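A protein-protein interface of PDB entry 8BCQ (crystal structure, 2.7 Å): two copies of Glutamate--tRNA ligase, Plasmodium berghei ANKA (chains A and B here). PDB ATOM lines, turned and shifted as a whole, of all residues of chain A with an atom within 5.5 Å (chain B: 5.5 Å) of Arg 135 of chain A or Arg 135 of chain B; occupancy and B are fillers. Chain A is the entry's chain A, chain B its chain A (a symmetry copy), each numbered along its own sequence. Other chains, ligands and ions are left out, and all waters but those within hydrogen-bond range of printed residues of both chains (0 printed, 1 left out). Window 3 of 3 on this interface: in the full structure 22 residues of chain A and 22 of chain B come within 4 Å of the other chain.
Ile 90 of chain A touches Asn 128 of chain B, and with the chains exchanged Asn 128 of chain A touches Ile 90 of chain B. Arg 135 of chain B touches its own counterpart, Arg 135 of chain A. Asn 136 of chain A touches its own counterpart, Asn 136 of chain B. Of the 4 pairs that touch across the chains among the printed residues, 4 have their exchanged pair printed and touching as well.
Of the 11 printed residues of chain B, 4 touch a printed residue of chain A. Along chain B the printed residues that touch a printed residue of chain A span positions 90 to 136. Hydrophobic or aromatic side chains of chain A that line the printed part of chain B: Ile 90.
OD1 of Asn 136 of chain B lies close to OD1 of Asn 136 of chain A (3.4 Å). NH2 of Arg 135 of chain A sits close to NH2 of Arg 135 of chain B (3.2 Å).
CG2 of Ile 90 of chain A touches OD1 of Asn 128 of chain B, at 3.4 Å. CG2 of Ile 90 of chain B touches OD1 of Asn 128 of chain A, 3.4 Å away.
Of chain B, only Arg 135 comes within 4 Å of Arg 135 of chain A. Arg 135 of chain B touches just one residue of chain A: Arg 135. Of the printed residues of chain B, Ile 90 of chain A touches Asn 128. Of the printed residues of chain B, Asn 128 of chain A touches Ile 90 (3.4 Å). Of the printed residues of chain A, Asn 128 of chain B touches Ile 90 (3.4 Å). Of the printed residues of chain B, Asn 136 of chain A touches Asn 136 (3.4 Å). Printed residues of chain A within 4 Å of Asn 136 of chain B: Asn 136. The nearest residue of chain A that does not touch Arg 135 of chain B is Asp 132 of chain A (4.9 Å).
The side-chain carboxylate of Asp 132 of chain A is in salt-bridge range of the guanidinium group of Arg 135 of chain A (3.7 Å). NH2 of Arg 135 of chain B lies within salt-bridge range of OD1 of Asp 132 of chain B (3.7 Å). OD2 of Asp 132 of chain B lies within hydrogen-bond range of ND2 of Asn 128 of chain B. The side-chain amide nitrogen (ND2) of Asn 128 of chain A lies within hydrogen-bond range of the side-chain carboxylate (OD2) of Asp 132 of chain A, at 2.9 Å.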
ATOM      1  N   LYS A  89     -13.078 -26.367  18.986  1.00  0.00           N
ATOM      2  CA  LYS A  89     -13.919 -25.557  19.860  1.00  0.00           C
ATOM      3  C   LYS A  89     -13.305 -24.202  20.181  1.00  0.00           C
ATOM      4  O   LYS A  89     -14.041 -23.267  20.516  1.00  0.00           O
ATOM      5  CB  LYS A  89     -14.200 -26.311  21.161  1.00  0.00           C
ATOM      6  CG  LYS A  89     -12.946 -26.758  21.894  1.00  0.00           C
ATOM      7  CD  LYS A  89     -13.279 -27.378  23.234  1.00  0.00           C
ATOM      8  CE  LYS A  89     -12.061 -28.029  23.867  1.00  0.00           C
ATOM      9  NZ  LYS A  89     -11.662 -29.265  23.139  1.00  0.00           N
ATOM     10  N   ILE A  90     -11.985 -24.070  20.089  1.00  0.00           N
ATOM     11  CA  ILE A  90     -11.301 -22.841  20.461  1.00  0.00           C
ATOM     12  C   ILE A  90     -10.985 -21.979  19.246  1.00  0.00           C
ATOM     13  O   ILE A  90     -11.176 -20.762  19.281  1.00  0.00           O
ATOM     14  CB  ILE A  90     -10.024 -23.167  21.261  1.00  0.00           C
ATOM     15  CG1 ILE A  90     -10.402 -23.847  22.574  1.00  0.00           C
ATOM     16  CG2 ILE A  90      -9.220 -21.905  21.528  1.00  0.00           C
ATOM     17  CD1 ILE A  90     -11.336 -23.026  23.416  1.00  0.00           C
ATOM     18  N   ASN A 128     -17.069 -19.914  27.392  1.00  0.00           N
ATOM     19  CA  ASN A 128     -15.951 -20.525  28.098  1.00  0.00           C
ATOM     20  C   ASN A 128     -16.430 -21.486  29.179  1.00  0.00           C
ATOM     21  O   ASN A 128     -15.738 -22.462  29.491  1.00  0.00           O
ATOM     22  CB  ASN A 128     -15.058 -19.438  28.699  1.00  0.00           C
ATOM     23  CG  ASN A 128     -13.900 -20.005  29.500  1.00  0.00           C
ATOM     24  OD1 ASN A 128     -12.889 -20.436  28.940  1.00  0.00           O
ATOM     25  ND2 ASN A 128     -14.041 -20.004  30.821  1.00  0.00           N
ATOM     26  N   TRP A 130     -19.097 -23.487  28.948  1.00  0.00           N
ATOM     27  CA  TRP A 130     -19.385 -24.743  28.265  1.00  0.00           C
ATOM     28  C   TRP A 130     -18.100 -25.479  27.910  1.00  0.00           C
ATOM     29  O   TRP A 130     -18.043 -26.713  27.974  1.00  0.00           O
ATOM     30  CB  TRP A 130     -20.224 -24.483  27.015  1.00  0.00           C
ATOM     31  CG  TRP A 130     -21.628 -24.052  27.322  1.00  0.00           C
ATOM     32  CD1 TRP A 130     -22.152 -22.801  27.184  1.00  0.00           C
ATOM     33  CD2 TRP A 130     -22.685 -24.875  27.830  1.00  0.00           C
ATOM     34  NE1 TRP A 130     -23.470 -22.794  27.570  1.00  0.00           N
ATOM     35  CE2 TRP A 130     -23.821 -24.056  27.971  1.00  0.00           C
ATOM     36  CE3 TRP A 130     -22.781 -26.226  28.179  1.00  0.00           C
ATOM     37  CZ2 TRP A 130     -25.039 -24.542  28.445  1.00  0.00           C
ATOM     38  CZ3 TRP A 130     -23.989 -26.708  28.647  1.00  0.00           C
ATOM     39  CH2 TRP A 130     -25.103 -25.867  28.775  1.00  0.00           C
ATOM     40  N   ILE A 131     -17.055 -24.737  27.536  1.00  0.00           N
ATOM     41  CA  ILE A 131     -15.758 -25.356  27.277  1.00  0.00           C
ATOM     42  C   ILE A 131     -15.228 -26.018  28.543  1.00  0.00           C
ATOM     43  O   ILE A 131     -14.777 -27.170  28.521  1.00  0.00           O
ATOM     44  CB  ILE A 131     -14.768 -24.316  26.724  1.00  0.00           C
ATOM     45  CG1 ILE A 131     -15.309 -23.698  25.433  1.00  0.00           C
ATOM     46  CG2 ILE A 131     -13.413 -24.950  26.476  1.00  0.00           C
ATOM     47  CD1 ILE A 131     -15.591 -24.707  24.343  1.00  0.00           C
ATOM     48  N   ASP A 132     -15.286 -25.305  29.672  1.00  0.00           N
ATOM     49  CA  ASP A 132     -14.817 -25.876  30.931  1.00  0.00           C
ATOM     50  C   ASP A 132     -15.686 -27.042  31.380  1.00  0.00           C
ATOM     51  O   ASP A 132     -15.188 -27.972  32.023  1.00  0.00           O
ATOM     52  CB  ASP A 132     -14.780 -24.805  32.020  1.00  0.00           C
ATOM     53  CG  ASP A 132     -13.810 -23.684  31.706  1.00  0.00           C
ATOM     54  OD1 ASP A 132     -12.808 -23.941  31.004  1.00  0.00           O
ATOM     55  OD2 ASP A 132     -14.049 -22.547  32.164  1.00  0.00           O
ATOM     56  N   PHE A 133     -16.979 -27.009  31.052  1.00  0.00           N
ATOM     57  CA  PHE A 133     -17.882 -28.074  31.477  1.00  0.00           C
ATOM     58  C   PHE A 133     -17.564 -29.394  30.788  1.00  0.00           C
ATOM     59  O   PHE A 133     -17.789 -30.462  31.367  1.00  0.00           O
ATOM     60  CB  PHE A 133     -19.331 -27.662  31.215  1.00  0.00           C
ATOM     61  CG  PHE A 133     -20.345 -28.659  31.699  1.00  0.00           C
ATOM     62  CD1 PHE A 133     -20.325 -29.105  33.010  1.00  0.00           C
ATOM     63  CD2 PHE A 133     -21.328 -29.137  30.848  1.00  0.00           C
ATOM     64  CE1 PHE A 133     -21.259 -30.018  33.460  1.00  0.00           C
ATOM     65  CE2 PHE A 133     -22.264 -30.050  31.291  1.00  0.00           C
ATOM     66  CZ  PHE A 133     -22.231 -30.490  32.600  1.00  0.00           C
ATOM     67  N   LEU A 134     -17.050 -29.348  29.560  1.00  0.00           N
ATOM     68  CA  LEU A 134     -16.684 -30.553  28.826  1.00  0.00           C
ATOM     69  C   LEU A 134     -15.179 -30.742  28.702  1.00  0.00           C
ATOM     70  O   LEU A 134     -14.742 -31.692  28.045  1.00  0.00           O
ATOM     71  CB  LEU A 134     -17.318 -30.534  27.430  1.00  0.00           C
ATOM     72  CG  LEU A 134     -18.839 -30.398  27.381  1.00  0.00           C
ATOM     73  CD1 LEU A 134     -19.345 -30.577  25.960  1.00  0.00           C
ATOM     74  CD2 LEU A 134     -19.493 -31.399  28.315  1.00  0.00           C
ATOM     75  N   ARG A 135     -14.379 -29.875  29.316  1.00  0.00           N
ATOM     76  CA  ARG A 135     -12.930 -29.974  29.202  1.00  0.00           C
ATOM     77  C   ARG A 135     -12.418 -31.191  29.964  1.00  0.00           C
ATOM     78  O   ARG A 135     -12.740 -31.379  31.141  1.00  0.00           O
ATOM     79  CB  ARG A 135     -12.272 -28.702  29.735  1.00  0.00           C
ATOM     80  CG  ARG A 135     -10.758 -28.696  29.650  1.00  0.00           C
ATOM     81  CD  ARG A 135     -10.273 -27.850  28.490  1.00  0.00           C
ATOM     82  NE  ARG A 135     -10.563 -26.436  28.692  1.00  0.00           N
ATOM     83  CZ  ARG A 135     -10.207 -25.470  27.855  1.00  0.00           C
ATOM     84  NH1 ARG A 135      -9.545 -25.732  26.740  1.00  0.00           N
ATOM     85  NH2 ARG A 135     -10.524 -24.212  28.144  1.00  0.00           N
ATOM     86  N   ASN A 136     -11.614 -32.014  29.286  1.00  0.00           N
ATOM     87  CA  ASN A 136     -10.990 -33.196  29.885  1.00  0.00           C
ATOM     88  C   ASN A 136     -12.031 -34.115  30.519  1.00  0.00           C
ATOM     89  O   ASN A 136     -11.812 -34.699  31.584  1.00  0.00           O
ATOM     90  CB  ASN A 136      -9.924 -32.795  30.907  1.00  0.00           C
ATOM     91  CG  ASN A 136      -8.818 -31.955  30.297  1.00  0.00           C
ATOM     92  OD1 ASN A 136      -8.536 -30.849  30.759  1.00  0.00           O
ATOM     93  ND2 ASN A 136      -8.184 -32.477  29.251  1.00  0.00           N
ATOM     94  N   LYS A 137     -13.178 -34.246  29.859  1.00  0.00           N
ATOM     95  CA  LYS A 137     -14.286 -35.044  30.367  1.00  0.00           C
ATOM     96  C   LYS A 137     -14.710 -36.036  29.296  1.00  0.00           C
ATOM     97  O   LYS A 137     -15.042 -35.637  28.175  1.00  0.00           O
ATOM     98  CB  LYS A 137     -15.462 -34.151  30.777  1.00  0.00           C
ATOM     99  CG  LYS A 137     -16.701 -34.909  31.217  1.00  0.00           C
ATOM    100  CD  LYS A 137     -17.796 -33.959  31.685  1.00  0.00           C
ATOM    101  CE  LYS A 137     -17.391 -33.226  32.958  1.00  0.00           C
ATOM    102  NZ  LYS A 137     -18.457 -32.304  33.445  1.00  0.00           N
ATOM    103  N   LYS B  89      -6.384 -15.867  33.667  1.00  0.00           N
ATOM    104  CA  LYS B  89      -5.745 -15.939  32.358  1.00  0.00           C
ATOM    105  C   LYS B  89      -6.743 -15.894  31.210  1.00  0.00           C
ATOM    106  O   LYS B  89      -6.369 -15.509  30.097  1.00  0.00           O
ATOM    107  CB  LYS B  89      -4.908 -17.215  32.255  1.00  0.00           C
ATOM    108  CG  LYS B  89      -5.690 -18.487  32.536  1.00  0.00           C
ATOM    109  CD  LYS B  89      -4.848 -19.721  32.290  1.00  0.00           C
ATOM    110  CE  LYS B  89      -5.543 -20.979  32.784  1.00  0.00           C
ATOM    111  NZ  LYS B  89      -5.590 -21.030  34.271  1.00  0.00           N
ATOM    112  N   ILE B  90      -7.995 -16.272  31.448  1.00  0.00           N
ATOM    113  CA  ILE B  90      -8.997 -16.346  30.395  1.00  0.00           C
ATOM    114  C   ILE B  90      -9.888 -15.112  30.372  1.00  0.00           C
ATOM    115  O   ILE B  90     -10.178 -14.575  29.302  1.00  0.00           O
ATOM    116  CB  ILE B  90      -9.831 -17.634  30.547  1.00  0.00           C
ATOM    117  CG1 ILE B  90      -8.933 -18.852  30.354  1.00  0.00           C
ATOM    118  CG2 ILE B  90     -10.976 -17.654  29.547  1.00  0.00           C
ATOM    119  CD1 ILE B  90      -8.221 -18.859  29.030  1.00  0.00           C
ATOM    120  N   ASN B 128      -3.389 -18.685  23.116  1.00  0.00           N
ATOM    121  CA  ASN B 128      -3.993 -19.950  23.517  1.00  0.00           C
ATOM    122  C   ASN B 128      -2.949 -21.050  23.653  1.00  0.00           C
ATOM    123  O   ASN B 128      -3.121 -21.970  24.460  1.00  0.00           O
ATOM    124  CB  ASN B 128      -5.074 -20.351  22.511  1.00  0.00           C
ATOM    125  CG  ASN B 128      -5.709 -21.692  22.836  1.00  0.00           C
ATOM    126  OD1 ASN B 128      -6.575 -21.791  23.709  1.00  0.00           O
ATOM    127  ND2 ASN B 128      -5.283 -22.732  22.128  1.00  0.00           N
ATOM    128  N   TRP B 130       0.155 -20.641  24.823  1.00  0.00           N
ATOM    129  CA  TRP B 130       0.741 -20.472  26.148  1.00  0.00           C
ATOM    130  C   TRP B 130      -0.206 -20.972  27.231  1.00  0.00           C
ATOM    131  O   TRP B 130       0.233 -21.547  28.235  1.00  0.00           O
ATOM    132  CB  TRP B 130       1.107 -19.007  26.380  1.00  0.00           C
ATOM    133  CG  TRP B 130       2.266 -18.547  25.546  1.00  0.00           C
ATOM    134  CD1 TRP B 130       2.221 -17.724  24.460  1.00  0.00           C
ATOM    135  CD2 TRP B 130       3.644 -18.894  25.729  1.00  0.00           C
ATOM    136  NE1 TRP B 130       3.485 -17.532  23.959  1.00  0.00           N
ATOM    137  CE2 TRP B 130       4.377 -18.241  24.719  1.00  0.00           C
ATOM    138  CE3 TRP B 130       4.330 -19.693  26.649  1.00  0.00           C
ATOM    139  CZ2 TRP B 130       5.761 -18.361  24.604  1.00  0.00           C
ATOM    140  CZ3 TRP B 130       5.702 -19.810  26.535  1.00  0.00           C
ATOM    141  CH2 TRP B 130       6.403 -19.147  25.519  1.00  0.00           C
ATOM    142  N   ILE B 131      -1.511 -20.764  27.045  1.00  0.00           N
ATOM    143  CA  ILE B 131      -2.491 -21.299  27.985  1.00  0.00           C
ATOM    144  C   ILE B 131      -2.423 -22.822  28.009  1.00  0.00           C
ATOM    145  O   ILE B 131      -2.387 -23.443  29.077  1.00  0.00           O
ATOM    146  CB  ILE B 131      -3.903 -20.801  27.630  1.00  0.00           C
ATOM    147  CG1 ILE B 131      -3.951 -19.271  27.654  1.00  0.00           C
ATOM    148  CG2 ILE B 131      -4.927 -21.375  28.591  1.00  0.00           C
ATOM    149  CD1 ILE B 131      -3.558 -18.668  28.984  1.00  0.00           C
ATOM    150  N   ASP B 132      -2.389 -23.446  26.828  1.00  0.00           N
ATOM    151  CA  ASP B 132      -2.302 -24.902  26.764  1.00  0.00           C
ATOM    152  C   ASP B 132      -0.973 -25.412  27.304  1.00  0.00           C
ATOM    153  O   ASP B 132      -0.914 -26.513  27.861  1.00  0.00           O
ATOM    154  CB  ASP B 132      -2.501 -25.386  25.329  1.00  0.00           C
ATOM    155  CG  ASP B 132      -3.871 -25.045  24.780  1.00  0.00           C
ATOM    156  OD1 ASP B 132      -4.827 -24.953  25.579  1.00  0.00           O
ATOM    157  OD2 ASP B 132      -3.991 -24.873  23.549  1.00  0.00           O
ATOM    158  N   PHE B 133       0.096 -24.629  27.150  1.00  0.00           N
ATOM    159  CA  PHE B 133       1.410 -25.064  27.611  1.00  0.00           C
ATOM    160  C   PHE B 133       1.478 -25.150  29.130  1.00  0.00           C
ATOM    161  O   PHE B 133       2.223 -25.976  29.669  1.00  0.00           O
ATOM    162  CB  PHE B 133       2.489 -24.121  27.074  1.00  0.00           C
ATOM    163  CG  PHE B 133       3.889 -24.536  27.423  1.00  0.00           C
ATOM    164  CD1 PHE B 133       4.342 -25.811  27.128  1.00  0.00           C
ATOM    165  CD2 PHE B 133       4.759 -23.645  28.030  1.00  0.00           C
ATOM    166  CE1 PHE B 133       5.631 -26.194  27.443  1.00  0.00           C
ATOM    167  CE2 PHE B 133       6.048 -24.022  28.347  1.00  0.00           C
ATOM    168  CZ  PHE B 133       6.486 -25.298  28.052  1.00  0.00           C
ATOM    169  N   LEU B 134       0.721 -24.311  29.836  1.00  0.00           N
ATOM    170  CA  LEU B 134       0.692 -24.332  31.292  1.00  0.00           C
ATOM    171  C   LEU B 134      -0.610 -24.885  31.855  1.00  0.00           C
ATOM    172  O   LEU B 134      -0.784 -24.893  33.078  1.00  0.00           O
ATOM    173  CB  LEU B 134       0.934 -22.922  31.846  1.00  0.00           C
ATOM    174  CG  LEU B 134       2.231 -22.240  31.412  1.00  0.00           C
ATOM    175  CD1 LEU B 134       2.429 -20.940  32.171  1.00  0.00           C
ATOM    176  CD2 LEU B 134       3.414 -23.168  31.617  1.00  0.00           C
ATOM    177  N   ARG B 135      -1.520 -25.352  31.004  1.00  0.00           N
ATOM    178  CA  ARG B 135      -2.803 -25.856  31.475  1.00  0.00           C
ATOM    179  C   ARG B 135      -2.620 -27.177  32.211  1.00  0.00           C
ATOM    180  O   ARG B 135      -1.990 -28.105  31.692  1.00  0.00           O
ATOM    181  CB  ARG B 135      -3.761 -26.036  30.298  1.00  0.00           C
ATOM    182  CG  ARG B 135      -5.136 -26.547  30.680  1.00  0.00           C
ATOM    183  CD  ARG B 135      -6.160 -25.429  30.681  1.00  0.00           C
ATOM    184  NE  ARG B 135      -6.399 -24.912  29.339  1.00  0.00           N
ATOM    185  CZ  ARG B 135      -7.280 -23.964  29.047  1.00  0.00           C
ATOM    186  NH1 ARG B 135      -8.025 -23.401  29.985  1.00  0.00           N
ATOM    187  NH2 ARG B 135      -7.415 -23.572  27.784  1.00  0.00           N
ATOM    188  N   ASN B 136      -3.175 -27.258  33.422  1.00  0.00           N
ATOM    189  CA  ASN B 136      -3.141 -28.474  34.239  1.00  0.00           C
ATOM    190  C   ASN B 136      -1.712 -28.971  34.440  1.00  0.00           C
ATOM    191  O   ASN B 136      -1.440 -30.174  34.430  1.00  0.00           O
ATOM    192  CB  ASN B 136      -4.017 -29.570  33.627  1.00  0.00           C
ATOM    193  CG  ASN B 136      -5.469 -29.150  33.493  1.00  0.00           C
ATOM    194  OD1 ASN B 136      -6.041 -29.193  32.404  1.00  0.00           O
ATOM    195  ND2 ASN B 136      -6.071 -28.739  34.604  1.00  0.00           N
ATOM    196  N   LYS B 137      -0.786 -28.034  34.625  1.00  0.00           N
ATOM    197  CA  LYS B 137       0.629 -28.352  34.775  1.00  0.00           C
ATOM    198  C   LYS B 137       1.146 -27.702  36.048  1.00  0.00           C
ATOM    199  O   LYS B 137       1.034 -26.484  36.214  1.00  0.00           O
ATOM    200  CB  LYS B 137       1.429 -27.877  33.558  1.00  0.00           C
ATOM    201  CG  LYS B 137       2.930 -28.072  33.680  1.00  0.00           C
ATOM    202  CD  LYS B 137       3.648 -27.653  32.404  1.00  0.00           C
ATOM    203  CE  LYS B 137       3.292 -28.568  31.239  1.00  0.00           C
ATOM    204  NZ  LYS B 137       4.003 -28.187  29.983  1.00  0.00           N
